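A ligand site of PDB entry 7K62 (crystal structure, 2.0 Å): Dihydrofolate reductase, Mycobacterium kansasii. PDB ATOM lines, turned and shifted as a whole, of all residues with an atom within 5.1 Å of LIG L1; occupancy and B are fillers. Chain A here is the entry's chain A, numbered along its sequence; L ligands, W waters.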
ATOM      1  N   ILE A  13      -9.741 -20.541  26.313  1.00  0.00           N
ATOM      2  CA  ILE A  13      -8.806 -21.160  25.398  1.00  0.00           C
ATOM      3  C   ILE A  13      -8.369 -22.505  25.981  1.00  0.00           C
ATOM      4  O   ILE A  13      -7.930 -22.581  27.130  1.00  0.00           O
ATOM      5  CB  ILE A  13      -7.601 -20.239  25.107  1.00  0.00           C
ATOM      6  CG1 ILE A  13      -6.682 -20.841  24.041  1.00  0.00           C
ATOM      7  CG2 ILE A  13      -6.821 -19.904  26.383  1.00  0.00           C
ATOM      8  CD1 ILE A  13      -5.557 -19.901  23.623  1.00  0.00           C
ATOM      9  N   TRP A  14      -8.525 -23.562  25.178  1.00  0.00           N
ATOM     10  CA  TRP A  14      -8.141 -24.900  25.591  1.00  0.00           C
ATOM     11  C   TRP A  14      -7.700 -25.685  24.377  1.00  0.00           C
ATOM     12  O   TRP A  14      -7.976 -25.308  23.224  1.00  0.00           O
ATOM     13  CB  TRP A  14      -9.292 -25.623  26.322  1.00  0.00           C
ATOM     14  CG  TRP A  14     -10.464 -26.104  25.474  1.00  0.00           C
ATOM     15  CD1 TRP A  14     -10.548 -27.291  24.794  1.00  0.00           C
ATOM     16  CD2 TRP A  14     -11.715 -25.430  25.254  1.00  0.00           C
ATOM     17  NE1 TRP A  14     -11.771 -27.381  24.151  1.00  0.00           N
ATOM     18  CE2 TRP A  14     -12.500 -26.260  24.418  1.00  0.00           C
ATOM     19  CE3 TRP A  14     -12.238 -24.202  25.666  1.00  0.00           C
ATOM     20  CZ2 TRP A  14     -13.792 -25.885  23.987  1.00  0.00           C
ATOM     21  CZ3 TRP A  14     -13.529 -23.844  25.235  1.00  0.00           C
ATOM     22  CH2 TRP A  14     -14.277 -24.689  24.411  1.00  0.00           C
ATOM     23  N   ALA A  15      -7.013 -26.797  24.643  1.00  0.00           N
ATOM     24  CA  ALA A  15      -6.706 -27.822  23.662  1.00  0.00           C
ATOM     25  C   ALA A  15      -7.395 -29.094  24.119  1.00  0.00           C
ATOM     26  O   ALA A  15      -7.458 -29.372  25.323  1.00  0.00           O
ATOM     27  CB  ALA A  15      -5.192 -28.043  23.549  1.00  0.00           C
ATOM     28  N   ILE A  28      -1.623 -32.547  30.646  1.00  0.00           N
ATOM     29  CA  ILE A  28      -2.187 -32.568  29.307  1.00  0.00           C
ATOM     30  C   ILE A  28      -1.584 -33.771  28.587  1.00  0.00           C
ATOM     31  O   ILE A  28      -0.372 -33.764  28.313  1.00  0.00           O
ATOM     32  CB  ILE A  28      -1.893 -31.275  28.548  1.00  0.00           C
ATOM     33  CG1 ILE A  28      -2.521 -30.090  29.294  1.00  0.00           C
ATOM     34  CG2 ILE A  28      -2.354 -31.419  27.101  1.00  0.00           C
ATOM     35  CD1 ILE A  28      -1.998 -28.728  28.897  1.00  0.00           C
ATOM     36  N   ASP A  35       0.933 -26.116  19.696  1.00  0.00           N
ATOM     37  CA  ASP A  35      -0.147 -25.608  20.545  1.00  0.00           C
ATOM     38  C   ASP A  35       0.399 -24.705  21.640  1.00  0.00           C
ATOM     39  O   ASP A  35      -0.245 -23.714  22.006  1.00  0.00           O
ATOM     40  CB  ASP A  35      -0.957 -26.739  21.171  1.00  0.00           C
ATOM     41  CG  ASP A  35      -2.042 -26.212  22.105  1.00  0.00           C
ATOM     42  OD1 ASP A  35      -2.957 -25.464  21.627  1.00  0.00           O
ATOM     43  OD2 ASP A  35      -1.961 -26.502  23.318  1.00  0.00           O
ATOM     44  N   LEU A  36       1.568 -25.050  22.200  1.00  0.00           N
ATOM     45  CA  LEU A  36       2.222 -24.111  23.104  1.00  0.00           C
ATOM     46  C   LEU A  36       2.445 -22.764  22.404  1.00  0.00           C
ATOM     47  O   LEU A  36       2.126 -21.702  22.967  1.00  0.00           O
ATOM     48  CB  LEU A  36       3.534 -24.684  23.648  1.00  0.00           C
ATOM     49  CG  LEU A  36       4.215 -23.639  24.534  1.00  0.00           C
ATOM     50  CD1 LEU A  36       3.227 -23.096  25.557  1.00  0.00           C
ATOM     51  CD2 LEU A  36       5.486 -24.197  25.256  1.00  0.00           C
ATOM     52  N   HIS A  38       0.772 -21.534  19.904  1.00  0.00           N
ATOM     53  CA  HIS A  38      -0.553 -20.947  19.662  1.00  0.00           C
ATOM     54  C   HIS A  38      -1.126 -20.348  20.943  1.00  0.00           C
ATOM     55  O   HIS A  38      -1.622 -19.219  20.940  1.00  0.00           O
ATOM     56  CB  HIS A  38      -1.441 -22.043  19.067  1.00  0.00           C
ATOM     57  CG  HIS A  38      -2.896 -21.664  18.910  1.00  0.00           C
ATOM     58  ND1 HIS A  38      -3.367 -20.963  17.826  1.00  0.00           N
ATOM     59  CD2 HIS A  38      -3.975 -21.964  19.671  1.00  0.00           C
ATOM     60  CE1 HIS A  38      -4.677 -20.809  17.939  1.00  0.00           C
ATOM     61  NE2 HIS A  38      -5.078 -21.408  19.051  1.00  0.00           N
ATOM     62  N   PHE A  39      -1.012 -21.091  22.061  1.00  0.00           N
ATOM     63  CA  PHE A  39      -1.477 -20.588  23.364  1.00  0.00           C
ATOM     64  C   PHE A  39      -0.769 -19.303  23.766  1.00  0.00           C
ATOM     65  O   PHE A  39      -1.413 -18.343  24.219  1.00  0.00           O
ATOM     66  CB  PHE A  39      -1.271 -21.673  24.441  1.00  0.00           C
ATOM     67  CG  PHE A  39      -1.559 -21.201  25.842  1.00  0.00           C
ATOM     68  CD1 PHE A  39      -2.864 -20.978  26.268  1.00  0.00           C
ATOM     69  CD2 PHE A  39      -0.516 -20.976  26.735  1.00  0.00           C
ATOM     70  CE1 PHE A  39      -3.118 -20.553  27.567  1.00  0.00           C
ATOM     71  CE2 PHE A  39      -0.764 -20.539  28.037  1.00  0.00           C
ATOM     72  CZ  PHE A  39      -2.083 -20.329  28.448  1.00  0.00           C
ATOM     73  N   LYS A  40       0.560 -19.243  23.615  1.00  0.00           N
ATOM     74  CA  LYS A  40       1.283 -18.016  23.960  1.00  0.00           C
ATOM     75  C   LYS A  40       0.868 -16.866  23.048  1.00  0.00           C
ATOM     76  O   LYS A  40       0.765 -15.723  23.498  1.00  0.00           O
ATOM     77  CB  LYS A  40       2.799 -18.254  23.871  1.00  0.00           C
ATOM     78  CG  LYS A  40       3.421 -19.023  25.032  1.00  0.00           C
ATOM     79  CD  LYS A  40       4.863 -19.443  24.668  1.00  0.00           C
ATOM     80  CE  LYS A  40       5.719 -19.759  25.861  1.00  0.00           C
ATOM     81  NZ  LYS A  40       7.027 -20.347  25.436  1.00  0.00           N
ATOM     82  N   THR A  54      -4.983 -26.178  37.775  1.00  0.00           N
ATOM     83  CA  THR A  54      -4.208 -25.838  36.584  1.00  0.00           C
ATOM     84  C   THR A  54      -2.917 -25.115  36.946  1.00  0.00           C
ATOM     85  O   THR A  54      -1.869 -25.351  36.342  1.00  0.00           O
ATOM     86  CB  THR A  54      -5.071 -25.010  35.617  1.00  0.00           C
ATOM     87  OG1 THR A  54      -6.114 -25.848  35.103  1.00  0.00           O
ATOM     88  CG2 THR A  54      -4.236 -24.492  34.441  1.00  0.00           C
ATOM     89  N   SER A  57      -0.574 -27.670  37.864  1.00  0.00           N
ATOM     90  CA  SER A  57      -0.100 -28.462  36.730  1.00  0.00           C
ATOM     91  C   SER A  57       1.001 -27.779  35.942  1.00  0.00           C
ATOM     92  O   SER A  57       1.661 -28.437  35.134  1.00  0.00           O
ATOM     93  CB  SER A  57      -1.246 -28.789  35.777  1.00  0.00           C
ATOM     94  OG  SER A  57      -1.588 -27.646  34.996  1.00  0.00           O
ATOM     95  N   LEU A  58       1.169 -26.464  36.110  1.00  0.00           N
ATOM     96  CA  LEU A  58       2.200 -25.756  35.366  1.00  0.00           C
ATOM     97  C   LEU A  58       3.585 -26.222  35.828  1.00  0.00           C
ATOM     98  O   LEU A  58       3.766 -26.546  37.005  1.00  0.00           O
ATOM     99  CB  LEU A  58       2.080 -24.258  35.570  1.00  0.00           C
ATOM    100  CG  LEU A  58       0.889 -23.594  34.906  1.00  0.00           C
ATOM    101  CD1 LEU A  58       0.836 -22.165  35.327  1.00  0.00           C
ATOM    102  CD2 LEU A  58       1.083 -23.699  33.427  1.00  0.00           C
ATOM    103  N   PRO A  59       4.554 -26.293  34.924  1.00  0.00           N
ATOM    104  CA  PRO A  59       5.939 -26.563  35.363  1.00  0.00           C
ATOM    105  C   PRO A  59       6.486 -25.348  36.095  1.00  0.00           C
ATOM    106  O   PRO A  59       6.148 -24.207  35.768  1.00  0.00           O
ATOM    107  CB  PRO A  59       6.678 -26.815  34.056  1.00  0.00           C
ATOM    108  CG  PRO A  59       5.921 -26.010  33.056  1.00  0.00           C
ATOM    109  CD  PRO A  59       4.457 -26.175  33.464  1.00  0.00           C
ATOM    110  N   ALA A  62       7.227 -22.122  34.528  1.00  0.00           N
ATOM    111  CA  ALA A  62       6.173 -21.282  33.981  1.00  0.00           C
ATOM    112  C   ALA A  62       5.161 -20.878  35.047  1.00  0.00           C
ATOM    113  O   ALA A  62       3.991 -20.624  34.732  1.00  0.00           O
ATOM    114  CB  ALA A  62       5.459 -21.962  32.817  1.00  0.00           C
ATOM    115  N   LEU A  65       2.893 -17.715  34.684  1.00  0.00           N
ATOM    116  CA  LEU A  65       3.049 -17.659  33.233  1.00  0.00           C
ATOM    117  C   LEU A  65       3.602 -16.295  32.858  1.00  0.00           C
ATOM    118  O   LEU A  65       2.976 -15.280  33.194  1.00  0.00           O
ATOM    119  CB  LEU A  65       1.706 -17.887  32.544  1.00  0.00           C
ATOM    120  CG  LEU A  65       1.084 -19.260  32.813  1.00  0.00           C
ATOM    121  CD1 LEU A  65      -0.320 -19.313  32.268  1.00  0.00           C
ATOM    122  CD2 LEU A  65       1.908 -20.318  32.157  1.00  0.00           C
ATOM    123  N   PRO A  66       4.760 -16.217  32.217  1.00  0.00           N
ATOM    124  CA  PRO A  66       5.398 -14.910  32.036  1.00  0.00           C
ATOM    125  C   PRO A  66       4.650 -14.041  31.025  1.00  0.00           C
ATOM    126  O   PRO A  66       3.987 -14.529  30.117  1.00  0.00           O
ATOM    127  CB  PRO A  66       6.815 -15.260  31.556  1.00  0.00           C
ATOM    128  CG  PRO A  66       6.702 -16.641  31.011  1.00  0.00           C
ATOM    129  CD  PRO A  66       5.637 -17.327  31.802  1.00  0.00           C
ATOM    130  N   ARG A  68       2.029 -12.297  31.367  1.00  0.00           N
ATOM    131  CA  ARG A  68       0.589 -12.284  31.526  1.00  0.00           C
ATOM    132  C   ARG A  68       0.279 -12.049  32.994  1.00  0.00           C
ATOM    133  O   ARG A  68       1.044 -12.440  33.880  1.00  0.00           O
ATOM    134  CB  ARG A  68      -0.022 -13.606  31.039  1.00  0.00           C
ATOM    135  CG  ARG A  68       0.069 -13.788  29.531  1.00  0.00           C
ATOM    136  CD  ARG A  68       0.169 -15.260  29.118  1.00  0.00           C
ATOM    137  NE  ARG A  68       1.537 -15.750  29.247  1.00  0.00           N
ATOM    138  CZ  ARG A  68       1.961 -16.954  28.880  1.00  0.00           C
ATOM    139  NH1 ARG A  68       1.128 -17.852  28.360  1.00  0.00           N
ATOM    140  NH2 ARG A  68       3.242 -17.275  29.044  1.00  0.00           N
ATOM    141  N   ILE A 103      -7.955 -20.106  31.103  1.00  0.00           N
ATOM    142  CA  ILE A 103      -7.020 -21.055  30.527  1.00  0.00           C
ATOM    143  C   ILE A 103      -7.168 -22.459  31.107  1.00  0.00           C
ATOM    144  O   ILE A 103      -6.344 -23.332  30.800  1.00  0.00           O
ATOM    145  CB  ILE A 103      -5.570 -20.560  30.660  1.00  0.00           C
ATOM    146  CG1 ILE A 103      -5.168 -20.471  32.125  1.00  0.00           C
ATOM    147  CG2 ILE A 103      -5.382 -19.202  29.990  1.00  0.00           C
ATOM    148  CD1 ILE A 103      -3.692 -20.210  32.310  1.00  0.00           C
ATOM    149  N   GLY A 104      -8.205 -22.726  31.904  1.00  0.00           N
ATOM    150  CA  GLY A 104      -8.453 -24.045  32.457  1.00  0.00           C
ATOM    151  C   GLY A 104      -8.443 -24.069  33.984  1.00  0.00           C
ATOM    152  O   GLY A 104      -8.097 -23.091  34.645  1.00  0.00           O
ATOM    153  N   TYR A 109     -13.512 -23.597  33.178  1.00  0.00           N
ATOM    154  CA  TYR A 109     -14.223 -23.469  31.915  1.00  0.00           C
ATOM    155  C   TYR A 109     -15.728 -23.504  32.136  1.00  0.00           C
ATOM    156  O   TYR A 109     -16.460 -22.621  31.680  1.00  0.00           O
ATOM    157  CB  TYR A 109     -13.817 -24.584  30.952  1.00  0.00           C
ATOM    158  CG  TYR A 109     -12.405 -24.490  30.423  1.00  0.00           C
ATOM    159  CD1 TYR A 109     -11.831 -23.273  30.122  1.00  0.00           C
ATOM    160  CD2 TYR A 109     -11.655 -25.643  30.229  1.00  0.00           C
ATOM    161  CE1 TYR A 109     -10.517 -23.191  29.615  1.00  0.00           C
ATOM    162  CE2 TYR A 109     -10.332 -25.577  29.735  1.00  0.00           C
ATOM    163  CZ  TYR A 109      -9.786 -24.355  29.443  1.00  0.00           C
ATOM    164  OH  TYR A 109      -8.511 -24.299  28.956  1.00  0.00           O
ATOM    165  N   GLU A 120     -11.114 -20.261  21.807  1.00  0.00           N
ATOM    166  CA  GLU A 120     -10.015 -20.647  20.928  1.00  0.00           C
ATOM    167  C   GLU A 120      -9.635 -22.073  21.283  1.00  0.00           C
ATOM    168  O   GLU A 120      -9.067 -22.327  22.354  1.00  0.00           O
ATOM    169  CB  GLU A 120      -8.845 -19.691  21.063  1.00  0.00           C
ATOM    170  CG  GLU A 120      -9.208 -18.283  20.621  1.00  0.00           C
ATOM    171  CD  GLU A 120      -9.357 -18.176  19.119  1.00  0.00           C
ATOM    172  OE1 GLU A 120      -8.887 -19.081  18.412  1.00  0.00           O
ATOM    173  OE2 GLU A 120      -9.949 -17.179  18.640  1.00  0.00           O
ATOM    174  N   THR A 122      -7.886 -25.780  20.328  1.00  0.00           N
ATOM    175  CA  THR A 122      -7.045 -26.679  19.539  1.00  0.00           C
ATOM    176  C   THR A 122      -7.646 -28.068  19.643  1.00  0.00           C
ATOM    177  O   THR A 122      -7.964 -28.528  20.749  1.00  0.00           O
ATOM    178  CB  THR A 122      -5.595 -26.711  20.035  1.00  0.00           C
ATOM    179  OG1 THR A 122      -5.054 -25.387  20.043  1.00  0.00           O
ATOM    180  CG2 THR A 122      -4.762 -27.603  19.115  1.00  0.00           C
HETATM  181  C1  LIG L   1      -4.732 -23.935  27.169  1.00  0.00           C
HETATM  182  N1  LIG L   1      -5.096 -23.829  25.883  1.00  0.00           N
HETATM  183  C2  LIG L   1      -4.284 -24.381  24.993  1.00  0.00           C
HETATM  184  N2  LIG L   1      -3.124 -25.037  25.262  1.00  0.00           N
HETATM  185  C3  LIG L   1      -2.767 -25.154  26.544  1.00  0.00           C
HETATM  186  C4  LIG L   1      -3.509 -24.613  27.517  1.00  0.00           C
HETATM  187  N3  LIG L   1      -5.489 -23.412  28.118  1.00  0.00           N
HETATM  188  N4  LIG L   1      -4.669 -24.271  23.704  1.00  0.00           N
HETATM  189  C5  LIG L   1      -1.462 -25.909  26.862  1.00  0.00           C
HETATM  190  C6  LIG L   1      -0.239 -25.110  26.349  1.00  0.00           C
HETATM  191  O1  LIG L   1      -3.142 -24.734  28.852  1.00  0.00           O
HETATM  192  C7  LIG L   1      -2.497 -23.634  29.546  1.00  0.00           C
HETATM  193  C8  LIG L   1      -1.989 -24.126  30.911  1.00  0.00           C
HETATM  194  C9  LIG L   1      -0.861 -25.163  30.766  1.00  0.00           C
HETATM  195  O2  LIG L   1       0.251 -24.564  30.054  1.00  0.00           O
HETATM  196  C10 LIG L   1       1.501 -25.174  29.949  1.00  0.00           C
HETATM  197  C11 LIG L   1       2.595 -24.393  29.538  1.00  0.00           C
HETATM  198  C12 LIG L   1       3.835 -25.037  29.458  1.00  0.00           C
HETATM  199  C13 LIG L   1       3.972 -26.384  29.755  1.00  0.00           C
HETATM  200  C14 LIG L   1       2.868 -27.133  30.152  1.00  0.00           C
HETATM  201  C15 LIG L   1       1.638 -26.521  30.245  1.00  0.00           C
HETATM  202  C16 LIG L   1       2.460 -22.913  29.204  1.00  0.00           C
HETATM  203  C17 LIG L   1       3.706 -21.990  29.250  1.00  0.00           C
HETATM  204  C18 LIG L   1       3.417 -20.590  28.601  1.00  0.00           C
HETATM  205  O3  LIG L   1       4.274 -19.681  28.672  1.00  0.00           O
HETATM  206  O4  LIG L   1       2.294 -20.508  28.040  1.00  0.00           O
HETATM  207  P1  LG2 L   2      -9.176 -26.652  37.625  1.00  0.00           P
HETATM  208  O1  LG2 L   2     -10.387 -26.136  36.909  1.00  0.00           O
HETATM  209  O2  LG2 L   2      -7.899 -26.192  36.917  1.00  0.00           O
HETATM  210  O3  LG2 L   2      -9.065 -26.182  39.164  1.00  0.00           O
HETATM  211  C1  LG2 L   2      -9.990 -26.696  40.137  1.00  0.00           C
HETATM  212  C2  LG2 L   2      -9.935 -25.863  41.388  1.00  0.00           C
HETATM  213  O4  LG2 L   2     -10.404 -24.527  41.114  1.00  0.00           O
HETATM  214  C3  LG2 L   2     -10.810 -26.350  42.528  1.00  0.00           C
HETATM  215  O5  LG2 L   2     -10.206 -27.449  43.212  1.00  0.00           O
HETATM  216  C4  LG2 L   2     -10.808 -25.072  43.365  1.00  0.00           C
HETATM  217  O6  LG2 L   2      -9.518 -24.954  43.987  1.00  0.00           O
HETATM  218  C5  LG2 L   2     -10.942 -23.981  42.309  1.00  0.00           C
HETATM  219  N1  LG2 L   2     -12.314 -23.542  42.068  1.00  0.00           N
HETATM  220  C6  LG2 L   2     -13.265 -24.161  41.299  1.00  0.00           C
HETATM  221  N2  LG2 L   2     -14.423 -23.543  41.285  1.00  0.00           N
HETATM  222  C7  LG2 L   2     -14.219 -22.448  42.096  1.00  0.00           C
HETATM  223  C8  LG2 L   2     -15.070 -21.400  42.508  1.00  0.00           C
HETATM  224  N3  LG2 L   2     -16.344 -21.265  42.109  1.00  0.00           N
HETATM  225  N4  LG2 L   2     -14.561 -20.467  43.355  1.00  0.00           N
HETATM  226  C9  LG2 L   2     -13.282 -20.584  43.741  1.00  0.00           C
HETATM  227  N5  LG2 L   2     -12.384 -21.516  43.416  1.00  0.00           N
HETATM  228  C10 LG2 L   2     -12.921 -22.432  42.595  1.00  0.00           C
HETATM  229  O7  LG2 L   2      -9.254 -28.237  37.700  1.00  0.00           O
HETATM  230  P2  LG2 L   2      -9.694 -29.390  36.682  1.00  0.00           P
HETATM  231  O8  LG2 L   2      -9.454 -30.708  37.307  1.00  0.00           O
HETATM  232  O9  LG2 L   2     -11.049 -29.092  36.170  1.00  0.00           O
HETATM  233  O10 LG2 L   2      -8.640 -29.140  35.519  1.00  0.00           O
HETATM  234  C11 LG2 L   2      -7.224 -29.358  35.705  1.00  0.00           C
HETATM  235  C12 LG2 L   2      -6.745 -30.343  34.669  1.00  0.00           C
HETATM  236  O11 LG2 L   2      -6.963 -29.806  33.355  1.00  0.00           O
HETATM  237  C13 LG2 L   2      -5.252 -30.721  34.750  1.00  0.00           C
HETATM  238  O12 LG2 L   2      -5.031 -32.105  34.470  1.00  0.00           O
HETATM  239  C14 LG2 L   2      -4.628 -29.857  33.649  1.00  0.00           C
HETATM  240  O13 LG2 L   2      -3.453 -30.458  33.110  1.00  0.00           O
HETATM  241  C15 LG2 L   2      -5.768 -29.821  32.621  1.00  0.00           C
HETATM  242  N6  LG2 L   2      -5.740 -28.586  31.719  1.00  0.00           N
HETATM  243  C16 LG2 L   2      -5.816 -28.769  30.388  1.00  0.00           C
HETATM  244  C17 LG2 L   2      -5.896 -27.673  29.542  1.00  0.00           C
HETATM  245  C18 LG2 L   2      -6.061 -27.833  28.055  1.00  0.00           C
HETATM  246  O14 LG2 L   2      -6.233 -26.843  27.352  1.00  0.00           O
HETATM  247  N7  LG2 L   2      -6.061 -29.071  27.552  1.00  0.00           N
HETATM  248  C19 LG2 L   2      -5.847 -26.401  30.093  1.00  0.00           C
HETATM  249  C20 LG2 L   2      -5.731 -26.243  31.468  1.00  0.00           C
HETATM  250  C21 LG2 L   2      -5.694 -27.360  32.268  1.00  0.00           C
HETATM  251  P3  LG2 L   2      -9.195 -25.536  45.472  1.00  0.00           P
HETATM  252  O15 LG2 L   2      -9.375 -27.000  45.544  1.00  0.00           O
HETATM  253  O16 LG2 L   2      -7.800 -25.052  45.752  1.00  0.00           O
HETATM  254  O17 LG2 L   2     -10.170 -24.776  46.368  1.00  0.00           O
HETATM  255  O   HOH W   1      -6.503 -23.196  21.447  1.00  0.00           O
HETATM  256  O   HOH W   2       6.894 -20.187  29.324  1.00  0.00           O
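An oxygen (O3) of LIG L1 is in salt-bridge range of the guanidinium group of Arg 68. OD2 of Asp 35 sits at hydrogen-bond distance from N2 of LIG L1. The backbone carbonyl oxygen (O) of Ile 13 sits at hydrogen-bond distance from a nitrogen (N3) of LIG L1. The backbone carbonyl oxygen (O) of Ile 103 lies within hydrogen-bond range of a nitrogen (N3) of LIG L1, at 2.8 Å. The backbone carbonyl oxygen of Trp 14 lies close to a nitrogen (N4) of LIG L1 (3.5 Å). The side-chain hydroxyl (OH) of Tyr 109 sits at hydrogen-bond distance from a nitrogen (N3) of LIG L1. An oxygen (O14) of LG2 L2 is in hydrogen-bond range of the backbone NH of Ala 15. N7 of LG2 L2 lies within hydrogen-bond range of O of Ala 15 (2.6 Å). The backbone NH (N) of Thr 54 is in hydrogen-bond range of an oxygen (O2) of LG2 L2, at 3.0 Å. OG1 of Thr 54 lies within hydrogen-bond range of O2 of LG2 L2 (2.6 Å).
Water W1 lies within hydrogen-bond range of O of Glu 120, OG1 of Thr 122, N4 of LIG L1, O of Trp 14 and NE2 of His 38.
N of Ala 15 touches N4 of LIG L1, at 3.6 Å. CD1 of Ile 28 touches C5 of LIG L1 (3.5 Å). Leu 36 touches LIG L1 (CD1 to O4, 3.7 Å). CE2 of Phe 39 touches O4 of LIG L1, at 3.1 Å. CE of Lys 40 touches O3 of LIG L1 (3.2 Å). Leu 58 touches LIG L1 (CD2 to O2, 3.6 Å). Pro 59 touches LIG L1 (CD to C13, 3.7 Å). Ala 62 touches LIG L1. CD2 of Leu 65 touches C17 of LIG L1 (3.8 Å). OG1 of Thr 122 touches N4 of LIG L1, at 3.8 Å. 16 residues have an atom within 4 Å of LIG L1: Ile 13, Trp 14, Ala 15, Ile 28, Asp 35, Leu 36, Phe 39, Lys 40, Leu 58, Pro 59, Ala 62, Leu 65, Arg 68, Ile 103, Tyr 109 and Thr 122.
NE of Arg 68 is in hydrogen-bond range of O of Pro 66, at 2.9 Å. OD1 of Asp 35 is in hydrogen-bond range of OG1 of Thr 122 (2.6 Å). The side-chain hydroxyl (OH) of Tyr 109 is in hydrogen-bond range of the backbone carbonyl oxygen (O) of Ile 13, 2.6 Å away. O of Ile 103 lies within hydrogen-bond range of OH of Tyr 109. O of Trp 14 is in hydrogen-bond range of N of Thr 122 (2.9 Å). The backbone carbonyl oxygen of Glu 120 sits at hydrogen-bond distance from the backbone NH of Trp 14 (3.1 Å). OH of Tyr 109 lies close to N of Gly 104, 3.4 Å away.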
